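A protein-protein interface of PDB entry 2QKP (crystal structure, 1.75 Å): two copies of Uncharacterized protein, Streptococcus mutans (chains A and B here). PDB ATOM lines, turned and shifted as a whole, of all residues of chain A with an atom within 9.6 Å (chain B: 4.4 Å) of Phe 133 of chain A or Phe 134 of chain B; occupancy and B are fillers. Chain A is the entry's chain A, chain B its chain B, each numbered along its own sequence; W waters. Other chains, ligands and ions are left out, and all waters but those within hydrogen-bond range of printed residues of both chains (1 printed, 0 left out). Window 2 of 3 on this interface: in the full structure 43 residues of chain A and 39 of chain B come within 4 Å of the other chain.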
ATOM      1  N   PRO A  29      -1.758 -24.604  24.148  1.00  0.00           N
ATOM      2  CA  PRO A  29      -1.640 -23.570  23.121  1.00  0.00           C
ATOM      3  C   PRO A  29      -2.380 -22.275  23.525  1.00  0.00           C
ATOM      4  O   PRO A  29      -3.134 -21.693  22.716  1.00  0.00           O
ATOM      5  CB  PRO A  29      -2.324 -24.237  21.916  1.00  0.00           C
ATOM      6  CG  PRO A  29      -3.403 -25.010  22.513  1.00  0.00           C
ATOM      7  CD  PRO A  29      -2.886 -25.503  23.860  1.00  0.00           C
ATOM      8  N   LEU A  30      -2.151 -21.826  24.758  1.00  0.00           N
ATOM      9  CA  LEU A  30      -2.922 -20.725  25.341  1.00  0.00           C
ATOM     10  C   LEU A  30      -1.989 -19.868  26.170  1.00  0.00           C
ATOM     11  O   LEU A  30      -1.088 -20.404  26.804  1.00  0.00           O
ATOM     12  CB  LEU A  30      -4.001 -21.262  26.287  1.00  0.00           C
ATOM     13  CG  LEU A  30      -5.017 -22.253  25.714  1.00  0.00           C
ATOM     14  CD1 LEU A  30      -5.813 -23.004  26.801  1.00  0.00           C
ATOM     15  CD2 LEU A  30      -5.972 -21.511  24.778  1.00  0.00           C
ATOM     16  N   TRP A  96     -12.976 -11.282  20.666  1.00  0.00           N
ATOM     17  CA  TRP A  96     -12.087 -11.724  19.602  1.00  0.00           C
ATOM     18  C   TRP A  96     -11.799 -10.547  18.674  1.00  0.00           C
ATOM     19  O   TRP A  96     -12.613  -9.613  18.575  1.00  0.00           O
ATOM     20  CB  TRP A  96     -12.684 -12.889  18.813  1.00  0.00           C
ATOM     21  CG  TRP A  96     -14.089 -12.665  18.301  1.00  0.00           C
ATOM     22  CD1 TRP A  96     -14.464 -12.102  17.104  1.00  0.00           C
ATOM     23  CD2 TRP A  96     -15.296 -13.030  18.965  1.00  0.00           C
ATOM     24  NE1 TRP A  96     -15.840 -12.086  16.994  1.00  0.00           N
ATOM     25  CE2 TRP A  96     -16.375 -12.659  18.121  1.00  0.00           C
ATOM     26  CE3 TRP A  96     -15.578 -13.609  20.198  1.00  0.00           C
ATOM     27  CZ2 TRP A  96     -17.707 -12.850  18.491  1.00  0.00           C
ATOM     28  CZ3 TRP A  96     -16.892 -13.832  20.544  1.00  0.00           C
ATOM     29  CH2 TRP A  96     -17.948 -13.449  19.697  1.00  0.00           C
ATOM     30  N   PHE A 105      -5.504 -14.406  14.713  1.00  0.00           N
ATOM     31  CA  PHE A 105      -6.839 -13.983  15.031  1.00  0.00           C
ATOM     32  C   PHE A 105      -7.067 -14.447  16.458  1.00  0.00           C
ATOM     33  O   PHE A 105      -7.067 -15.635  16.726  1.00  0.00           O
ATOM     34  CB  PHE A 105      -7.882 -14.582  14.104  1.00  0.00           C
ATOM     35  CG  PHE A 105      -9.191 -13.913  14.222  1.00  0.00           C
ATOM     36  CD1 PHE A 105      -9.473 -12.774  13.469  1.00  0.00           C
ATOM     37  CD2 PHE A 105     -10.117 -14.335  15.149  1.00  0.00           C
ATOM     38  CE1 PHE A 105     -10.691 -12.130  13.600  1.00  0.00           C
ATOM     39  CE2 PHE A 105     -11.352 -13.685  15.274  1.00  0.00           C
ATOM     40  CZ  PHE A 105     -11.632 -12.604  14.521  1.00  0.00           C
ATOM     41  N   VAL A 106      -7.256 -13.493  17.358  1.00  0.00           N
ATOM     42  CA  VAL A 106      -7.168 -13.776  18.785  1.00  0.00           C
ATOM     43  C   VAL A 106      -8.549 -14.008  19.374  1.00  0.00           C
ATOM     44  O   VAL A 106      -9.478 -13.230  19.121  1.00  0.00           O
ATOM     45  CB  VAL A 106      -6.474 -12.581  19.505  1.00  0.00           C
ATOM     46  CG1 VAL A 106      -6.359 -12.830  21.032  1.00  0.00           C
ATOM     47  CG2 VAL A 106      -5.072 -12.324  18.898  1.00  0.00           C
ATOM     48  N   TYR A 107      -8.694 -15.077  20.162  1.00  0.00           N
ATOM     49  CA  TYR A 107      -9.943 -15.330  20.876  1.00  0.00           C
ATOM     50  C   TYR A 107      -9.625 -15.358  22.368  1.00  0.00           C
ATOM     51  O   TYR A 107      -8.753 -16.127  22.803  1.00  0.00           O
ATOM     52  CB  TYR A 107     -10.475 -16.709  20.462  1.00  0.00           C
ATOM     53  CG  TYR A 107     -11.842 -17.040  21.026  1.00  0.00           C
ATOM     54  CD1 TYR A 107     -12.998 -16.591  20.394  1.00  0.00           C
ATOM     55  CD2 TYR A 107     -11.987 -17.840  22.163  1.00  0.00           C
ATOM     56  CE1 TYR A 107     -14.263 -16.905  20.888  1.00  0.00           C
ATOM     57  CE2 TYR A 107     -13.260 -18.144  22.680  1.00  0.00           C
ATOM     58  CZ  TYR A 107     -14.388 -17.688  22.021  1.00  0.00           C
ATOM     59  OH  TYR A 107     -15.657 -18.013  22.486  1.00  0.00           O
ATOM     60  N   VAL A 127      -5.976 -17.024  26.275  1.00  0.00           N
ATOM     61  CA  VAL A 127      -5.958 -16.401  24.965  1.00  0.00           C
ATOM     62  C   VAL A 127      -5.469 -17.444  23.955  1.00  0.00           C
ATOM     63  O   VAL A 127      -4.444 -18.100  24.176  1.00  0.00           O
ATOM     64  CB  VAL A 127      -4.999 -15.183  24.947  1.00  0.00           C
ATOM     65  CG1 VAL A 127      -4.986 -14.569  23.606  1.00  0.00           C
ATOM     66  CG2 VAL A 127      -5.365 -14.138  26.033  1.00  0.00           C
ATOM     67  N   GLN A 128      -6.187 -17.559  22.837  1.00  0.00           N
ATOM     68  CA  GLN A 128      -5.817 -18.540  21.815  1.00  0.00           C
ATOM     69  C   GLN A 128      -5.772 -17.903  20.434  1.00  0.00           C
ATOM     70  O   GLN A 128      -6.558 -17.014  20.118  1.00  0.00           O
ATOM     71  CB  GLN A 128      -6.828 -19.669  21.798  1.00  0.00           C
ATOM     72  CG  GLN A 128      -6.382 -20.928  20.963  1.00  0.00           C
ATOM     73  CD  GLN A 128      -7.364 -22.075  21.133  1.00  0.00           C
ATOM     74  OE1 GLN A 128      -8.444 -21.906  21.721  1.00  0.00           O
ATOM     75  NE2 GLN A 128      -7.008 -23.239  20.617  1.00  0.00           N
ATOM     76  N   ASP A 129      -4.856 -18.381  19.598  1.00  0.00           N
ATOM     77  CA  ASP A 129      -4.899 -17.986  18.199  1.00  0.00           C
ATOM     78  C   ASP A 129      -5.799 -19.001  17.471  1.00  0.00           C
ATOM     79  O   ASP A 129      -5.549 -20.223  17.463  1.00  0.00           O
ATOM     80  CB  ASP A 129      -3.488 -17.933  17.607  1.00  0.00           C
ATOM     81  CG  ASP A 129      -3.494 -17.731  16.100  1.00  0.00           C
ATOM     82  OD1 ASP A 129      -4.414 -17.055  15.569  1.00  0.00           O
ATOM     83  OD2 ASP A 129      -2.568 -18.288  15.450  1.00  0.00           O
ATOM     84  N   ILE A 130      -6.862 -18.487  16.866  1.00  0.00           N
ATOM     85  CA  ILE A 130      -7.805 -19.367  16.186  1.00  0.00           C
ATOM     86  C   ILE A 130      -7.718 -19.278  14.658  1.00  0.00           C
ATOM     87  O   ILE A 130      -8.431 -20.006  13.944  1.00  0.00           O
ATOM     88  CB  ILE A 130      -9.254 -19.181  16.675  1.00  0.00           C
ATOM     89  CG1 ILE A 130      -9.732 -17.737  16.477  1.00  0.00           C
ATOM     90  CG2 ILE A 130      -9.350 -19.515  18.150  1.00  0.00           C
ATOM     91  CD1 ILE A 130     -11.227 -17.548  16.596  1.00  0.00           C
ATOM     92  N   LYS A 131      -6.827 -18.424  14.163  1.00  0.00           N
ATOM     93  CA  LYS A 131      -6.623 -18.287  12.710  1.00  0.00           C
ATOM     94  C   LYS A 131      -6.366 -19.629  12.004  1.00  0.00           C
ATOM     95  O   LYS A 131      -6.949 -19.862  10.932  1.00  0.00           O
ATOM     96  CB  LYS A 131      -5.513 -17.275  12.380  1.00  0.00           C
ATOM     97  CG  LYS A 131      -5.343 -17.029  10.847  1.00  0.00           C
ATOM     98  CD  LYS A 131      -4.342 -15.943  10.565  1.00  0.00           C
ATOM     99  CE  LYS A 131      -4.715 -15.205   9.282  1.00  0.00           C
ATOM    100  NZ  LYS A 131      -5.838 -14.226   9.514  1.00  0.00           N
ATOM    101  N   PRO A 132      -5.511 -20.512  12.583  1.00  0.00           N
ATOM    102  CA  PRO A 132      -5.260 -21.830  11.975  1.00  0.00           C
ATOM    103  C   PRO A 132      -6.508 -22.661  11.711  1.00  0.00           C
ATOM    104  O   PRO A 132      -6.515 -23.441  10.752  1.00  0.00           O
ATOM    105  CB  PRO A 132      -4.358 -22.519  13.010  1.00  0.00           C
ATOM    106  CG  PRO A 132      -3.615 -21.385  13.632  1.00  0.00           C
ATOM    107  CD  PRO A 132      -4.687 -20.344  13.799  1.00  0.00           C
ATOM    108  N   PHE A 133      -7.556 -22.480  12.516  1.00  0.00           N
ATOM    109  CA  PHE A 133      -8.777 -23.284  12.387  1.00  0.00           C
ATOM    110  C   PHE A 133      -9.630 -22.875  11.194  1.00  0.00           C
ATOM    111  O   PHE A 133     -10.457 -23.664  10.727  1.00  0.00           O
ATOM    112  CB  PHE A 133      -9.639 -23.215  13.648  1.00  0.00           C
ATOM    113  CG  PHE A 133      -8.935 -23.683  14.893  1.00  0.00           C
ATOM    114  CD1 PHE A 133      -8.176 -24.847  14.880  1.00  0.00           C
ATOM    115  CD2 PHE A 133      -9.040 -22.977  16.074  1.00  0.00           C
ATOM    116  CE1 PHE A 133      -7.519 -25.277  16.011  1.00  0.00           C
ATOM    117  CE2 PHE A 133      -8.394 -23.430  17.214  1.00  0.00           C
ATOM    118  CZ  PHE A 133      -7.635 -24.576  17.173  1.00  0.00           C
ATOM    119  N   PHE A 134      -9.443 -21.645  10.718  1.00  0.00           N
ATOM    120  CA  PHE A 134     -10.231 -21.127   9.582  1.00  0.00           C
ATOM    121  C   PHE A 134      -9.952 -21.889   8.265  1.00  0.00           C
ATOM    122  O   PHE A 134     -10.746 -21.820   7.322  1.00  0.00           O
ATOM    123  CB  PHE A 134     -10.020 -19.609   9.397  1.00  0.00           C
ATOM    124  CG  PHE A 134     -10.450 -18.758  10.588  1.00  0.00           C
ATOM    125  CD1 PHE A 134      -9.857 -17.510  10.812  1.00  0.00           C
ATOM    126  CD2 PHE A 134     -11.436 -19.191  11.471  1.00  0.00           C
ATOM    127  CE1 PHE A 134     -10.252 -16.701  11.904  1.00  0.00           C
ATOM    128  CE2 PHE A 134     -11.836 -18.403  12.560  1.00  0.00           C
ATOM    129  CZ  PHE A 134     -11.247 -17.152  12.773  1.00  0.00           C
ATOM    130  N   GLU A 135      -8.837 -22.616   8.224  1.00  0.00           N
ATOM    131  CA  GLU A 135      -8.438 -23.431   7.064  1.00  0.00           C
ATOM    132  C   GLU A 135      -9.259 -24.718   6.974  1.00  0.00           C
ATOM    133  O   GLU A 135      -9.496 -25.255   5.874  1.00  0.00           O
ATOM    134  CB  GLU A 135      -6.951 -23.769   7.159  1.00  0.00           C
ATOM    135  CG  GLU A 135      -5.987 -22.590   6.874  1.00  0.00           C
ATOM    136  CD  GLU A 135      -6.571 -21.209   7.198  1.00  0.00           C
ATOM    137  OE1 GLU A 135      -6.898 -20.948   8.378  1.00  0.00           O
ATOM    138  OE2 GLU A 135      -6.706 -20.382   6.262  1.00  0.00           O
ATOM    139  N   LEU A 136      -9.710 -25.187   8.136  1.00  0.00           N
ATOM    140  CA  LEU A 136     -10.385 -26.473   8.264  1.00  0.00           C
ATOM    141  C   LEU A 136     -11.853 -26.361   7.899  1.00  0.00           C
ATOM    142  O   LEU A 136     -12.593 -27.345   7.947  1.00  0.00           O
ATOM    143  CB  LEU A 136     -10.223 -27.019   9.687  1.00  0.00           C
ATOM    144  CG  LEU A 136      -8.817 -26.907  10.276  1.00  0.00           C
ATOM    145  CD1 LEU A 136      -8.808 -27.368  11.715  1.00  0.00           C
ATOM    146  CD2 LEU A 136      -7.816 -27.690   9.457  1.00  0.00           C
ATOM    147  N   ASP A 137     -12.265 -25.153   7.529  1.00  0.00           N
ATOM    148  CA  ASP A 137     -13.596 -24.910   6.995  1.00  0.00           C
ATOM    149  C   ASP A 137     -13.955 -25.922   5.891  1.00  0.00           C
ATOM    150  O   ASP A 137     -15.059 -26.474   5.877  1.00  0.00           O
ATOM    151  CB  ASP A 137     -13.675 -23.479   6.452  1.00  0.00           C
ATOM    152  CG  ASP A 137     -15.072 -23.096   6.014  1.00  0.00           C
ATOM    153  OD1 ASP A 137     -16.007 -23.895   6.239  1.00  0.00           O
ATOM    154  OD2 ASP A 137     -15.235 -21.992   5.444  1.00  0.00           O
ATOM    155  N   SER A 138     -13.002 -26.177   4.996  1.00  0.00           N
ATOM    156  CA  SER A 138     -13.213 -27.044   3.834  1.00  0.00           C
ATOM    157  C   SER A 138     -13.514 -28.514   4.171  1.00  0.00           C
ATOM    158  O   SER A 138     -14.243 -29.178   3.438  1.00  0.00           O
ATOM    159  CB  SER A 138     -12.023 -26.935   2.867  1.00  0.00           C
ATOM    160  OG  SER A 138     -10.788 -26.813   3.563  1.00  0.00           O
ATOM    161  N   GLU A 139     -12.976 -29.008   5.283  1.00  0.00           N
ATOM    162  CA  GLU A 139     -13.089 -30.431   5.626  1.00  0.00           C
ATOM    163  C   GLU A 139     -14.295 -30.771   6.498  1.00  0.00           C
ATOM    164  O   GLU A 139     -14.430 -30.273   7.612  1.00  0.00           O
ATOM    165  CB  GLU A 139     -11.805 -30.918   6.288  1.00  0.00           C
ATOM    166  CG  GLU A 139     -10.674 -31.160   5.308  1.00  0.00           C
ATOM    167  CD  GLU A 139      -9.326 -31.083   5.976  1.00  0.00           C
ATOM    168  OE1 GLU A 139      -8.892 -29.959   6.311  1.00  0.00           O
ATOM    169  OE2 GLU A 139      -8.701 -32.146   6.170  1.00  0.00           O
ATOM    170  N   TYR B 107     -11.046 -31.124  17.328  1.00  0.00           N
ATOM    171  CA  TYR B 107      -9.670 -30.917  16.980  1.00  0.00           C
ATOM    172  C   TYR B 107      -8.800 -31.542  18.070  1.00  0.00           C
ATOM    173  O   TYR B 107      -8.884 -31.164  19.244  1.00  0.00           O
ATOM    174  CB  TYR B 107      -9.365 -29.423  16.804  1.00  0.00           C
ATOM    175  CG  TYR B 107      -8.018 -29.141  16.204  1.00  0.00           C
ATOM    176  CD1 TYR B 107      -7.842 -29.073  14.814  1.00  0.00           C
ATOM    177  CD2 TYR B 107      -6.905 -28.914  17.021  1.00  0.00           C
ATOM    178  CE1 TYR B 107      -6.595 -28.799  14.270  1.00  0.00           C
ATOM    179  CE2 TYR B 107      -5.682 -28.634  16.495  1.00  0.00           C
ATOM    180  CZ  TYR B 107      -5.524 -28.580  15.117  1.00  0.00           C
ATOM    181  OH  TYR B 107      -4.274 -28.311  14.599  1.00  0.00           O
ATOM    182  N   GLN B 128     -10.294 -30.291  21.603  1.00  0.00           N
ATOM    183  CA  GLN B 128     -11.048 -29.056  21.670  1.00  0.00           C
ATOM    184  C   GLN B 128     -12.209 -29.100  20.683  1.00  0.00           C
ATOM    185  O   GLN B 128     -12.097 -29.729  19.629  1.00  0.00           O
ATOM    186  CB  GLN B 128     -10.139 -27.895  21.304  1.00  0.00           C
ATOM    187  CG  GLN B 128     -10.768 -26.531  21.611  1.00  0.00           C
ATOM    188  CD  GLN B 128      -9.799 -25.378  21.430  1.00  0.00           C
ATOM    189  OE1 GLN B 128      -8.694 -25.534  20.905  1.00  0.00           O
ATOM    190  NE2 GLN B 128     -10.215 -24.205  21.880  1.00  0.00           N
ATOM    191  N   ILE B 130     -13.957 -26.970  18.117  1.00  0.00           N
ATOM    192  CA  ILE B 130     -13.641 -25.722  17.398  1.00  0.00           C
ATOM    193  C   ILE B 130     -14.833 -25.171  16.614  1.00  0.00           C
ATOM    194  O   ILE B 130     -14.722 -24.113  15.959  1.00  0.00           O
ATOM    195  CB  ILE B 130     -12.384 -25.825  16.491  1.00  0.00           C
ATOM    196  CG1 ILE B 130     -12.559 -26.858  15.363  1.00  0.00           C
ATOM    197  CG2 ILE B 130     -11.102 -26.013  17.329  1.00  0.00           C
ATOM    198  CD1 ILE B 130     -11.431 -26.795  14.297  1.00  0.00           C
ATOM    199  N   LYS B 131     -15.961 -25.872  16.682  1.00  0.00           N
ATOM    200  CA  LYS B 131     -17.180 -25.454  15.989  1.00  0.00           C
ATOM    201  C   LYS B 131     -17.578 -24.012  16.332  1.00  0.00           C
ATOM    202  O   LYS B 131     -17.883 -23.248  15.413  1.00  0.00           O
ATOM    203  CB  LYS B 131     -18.333 -26.427  16.255  1.00  0.00           C
ATOM    204  CG  LYS B 131     -19.595 -26.230  15.383  1.00  0.00           C
ATOM    205  CD  LYS B 131     -20.360 -27.574  15.309  1.00  0.00           C
ATOM    206  CE  LYS B 131     -21.848 -27.410  15.048  1.00  0.00           C
ATOM    207  NZ  LYS B 131     -22.120 -26.707  13.779  1.00  0.00           N
ATOM    208  N   PRO B 132     -17.555 -23.613  17.633  1.00  0.00           N
ATOM    209  CA  PRO B 132     -17.882 -22.217  17.953  1.00  0.00           C
ATOM    210  C   PRO B 132     -17.053 -21.163  17.209  1.00  0.00           C
ATOM    211  O   PRO B 132     -17.540 -20.050  17.021  1.00  0.00           O
ATOM    212  CB  PRO B 132     -17.610 -22.134  19.458  1.00  0.00           C
ATOM    213  CG  PRO B 132     -17.922 -23.549  19.950  1.00  0.00           C
ATOM    214  CD  PRO B 132     -17.291 -24.383  18.873  1.00  0.00           C
ATOM    215  N   PHE B 133     -15.832 -21.503  16.814  1.00  0.00           N
ATOM    216  CA  PHE B 133     -14.944 -20.549  16.160  1.00  0.00           C
ATOM    217  C   PHE B 133     -15.392 -20.299  14.737  1.00  0.00           C
ATOM    218  O   PHE B 133     -14.902 -19.378  14.081  1.00  0.00           O
ATOM    219  CB  PHE B 133     -13.511 -21.040  16.152  1.00  0.00           C
ATOM    220  CG  PHE B 133     -12.926 -21.208  17.536  1.00  0.00           C
ATOM    221  CD1 PHE B 133     -13.248 -20.309  18.552  1.00  0.00           C
ATOM    222  CD2 PHE B 133     -12.037 -22.225  17.805  1.00  0.00           C
ATOM    223  CE1 PHE B 133     -12.703 -20.461  19.851  1.00  0.00           C
ATOM    224  CE2 PHE B 133     -11.480 -22.368  19.093  1.00  0.00           C
ATOM    225  CZ  PHE B 133     -11.823 -21.484  20.104  1.00  0.00           C
ATOM    226  N   PHE B 134     -16.295 -21.154  14.255  1.00  0.00           N
ATOM    227  CA  PHE B 134     -16.881 -20.940  12.926  1.00  0.00           C
ATOM    228  C   PHE B 134     -18.248 -20.258  13.019  1.00  0.00           C
ATOM    229  O   PHE B 134     -18.939 -20.114  12.006  1.00  0.00           O
ATOM    230  CB  PHE B 134     -17.011 -22.280  12.204  1.00  0.00           C
ATOM    231  CG  PHE B 134     -15.721 -23.010  12.055  1.00  0.00           C
ATOM    232  CD1 PHE B 134     -15.521 -24.223  12.701  1.00  0.00           C
ATOM    233  CD2 PHE B 134     -14.678 -22.478  11.307  1.00  0.00           C
ATOM    234  CE1 PHE B 134     -14.328 -24.920  12.555  1.00  0.00           C
ATOM    235  CE2 PHE B 134     -13.472 -23.168  11.173  1.00  0.00           C
ATOM    236  CZ  PHE B 134     -13.306 -24.392  11.801  1.00  0.00           C
ATOM    237  N   GLU B 135     -18.651 -19.876  14.226  1.00  0.00           N
ATOM    238  CA  GLU B 135     -19.964 -19.277  14.485  1.00  0.00           C
ATOM    239  C   GLU B 135     -19.863 -17.934  15.202  1.00  0.00           C
ATOM    240  O   GLU B 135     -20.801 -17.513  15.863  1.00  0.00           O
ATOM    241  CB  GLU B 135     -20.832 -20.237  15.314  1.00  0.00           C
ATOM    242  CG  GLU B 135     -21.040 -21.599  14.664  1.00  0.00           C
ATOM    243  CD  GLU B 135     -21.829 -22.573  15.527  1.00  0.00           C
ATOM    244  OE1 GLU B 135     -21.821 -22.432  16.760  1.00  0.00           O
ATOM    245  OE2 GLU B 135     -22.457 -23.501  14.958  1.00  0.00           O
ATOM    246  N   LEU B 136     -18.727 -17.266  15.070  1.00  0.00           N
ATOM    247  CA  LEU B 136     -18.515 -15.988  15.766  1.00  0.00           C
ATOM    248  C   LEU B 136     -19.386 -14.885  15.193  1.00  0.00           C
ATOM    249  O   LEU B 136     -19.853 -14.016  15.920  1.00  0.00           O
ATOM    250  CB  LEU B 136     -17.051 -15.556  15.678  1.00  0.00           C
ATOM    251  CG  LEU B 136     -16.064 -16.582  16.258  1.00  0.00           C
ATOM    252  CD1 LEU B 136     -14.669 -16.054  16.136  1.00  0.00           C
ATOM    253  CD2 LEU B 136     -16.410 -16.879  17.703  1.00  0.00           C
HETATM  254  O   HOH W   1     -18.343 -11.092  15.222  1.00  0.00           O
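The side-chain amide oxygen (OE1) of Gln 128 of chain B sits at hydrogen-bond distance from the side-chain amide nitrogen (NE2) of Gln 128 of chain A (2.9 Å).
O of Phe 105 of chain A lies within hydrogen-bond range of N of Ile 130 of chain A, at 2.9 Å. The backbone carbonyl oxygen of Gln 128 of chain A is in hydrogen-bond range of the backbone NH of Tyr 107 of chain A, at 2.9 Å. The backbone carbonyl oxygen (O) of Tyr 107 of chain B is in hydrogen-bond range of the backbone NH (N) of Gln 128 of chain B, at 2.9 Å.
Among the printed residues, merely in contact across the chains: Phe 133 of chain A with Phe 134 of chain B (3.1 Å), Phe 133 of chain A with Phe 133 of chain B (3.5 Å), Trp 96 of chain A with Leu 136 of chain B (3.5 Å), Phe 134 of chain A with Phe 133 of chain B (3.6 Å), Tyr 107 of chain A with Phe 133 of chain B (3.6 Å), Leu 136 of chain A with Tyr 107 of chain B (3.7 Å), Ile 130 of chain A with Phe 133 of chain B (3.7 Å), Leu 136 of chain A with Ile 130 of chain B (3.7 Å), Phe 133 of chain A with Ile 130 of chain B (3.7 Å), Gln 128 of chain A with Phe 133 of chain B (3.8 Å), Ile 130 of chain A with Leu 136 of chain B (3.8 Å), Phe 133 of chain A with Tyr 107 of chain B (3.8 Å), Tyr 107 of chain A with Leu 136 of chain B (3.8 Å) and Phe 133 of chain A with Gln 128 of chain B (3.996 Å).
Of the printed residues of chain B, Ile 130 of chain A touches Phe 133 (3.7 Å) and Leu 136 (3.8 Å). Printed residues of chain B within 4 Å of Phe 133 of chain A: Tyr 107, Gln 128, Ile 130, Phe 133 and Phe 134. Of the printed residues of chain A, Tyr 107 of chain B touches Phe 133 and Leu 136. Of the printed residues of chain A, Phe 133 of chain B touches Tyr 107, Gln 128, Ile 130, Phe 133 and Phe 134. Of the printed residues of chain A, Leu 136 of chain B touches Trp 96 (3.5 Å), Tyr 107 (3.8 Å) and Ile 130 (3.8 Å).
Hydrophobic or aromatic side chains of chain B within 4 Å of the printed part of chain A: Tyr 107, Ile 130, Phe 133, Phe 134 and Leu 136. Of the 19 printed residues of chain A, 7 touch a printed residue of chain B. Among the printed residues, 15 pairs touch across the chains.
Tyr 107 of chain A touches Leu 136 of chain B, and with the chains exchanged Leu 136 of chain A touches Tyr 107 of chain B. Gln 128 of chain B touches its own counterpart, Gln 128 of chain A. Ile 130 of chain A touches Phe 133 of chain B, and with the chains exchanged Phe 133 of chain A touches Ile 130 of chain B. Phe 133 of chain A touches its own counterpart, Phe 133 of chain B.
Water W1 lies within hydrogen-bond range of NE1 of Trp 96 of chain A and O of Leu 136 of chain B.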
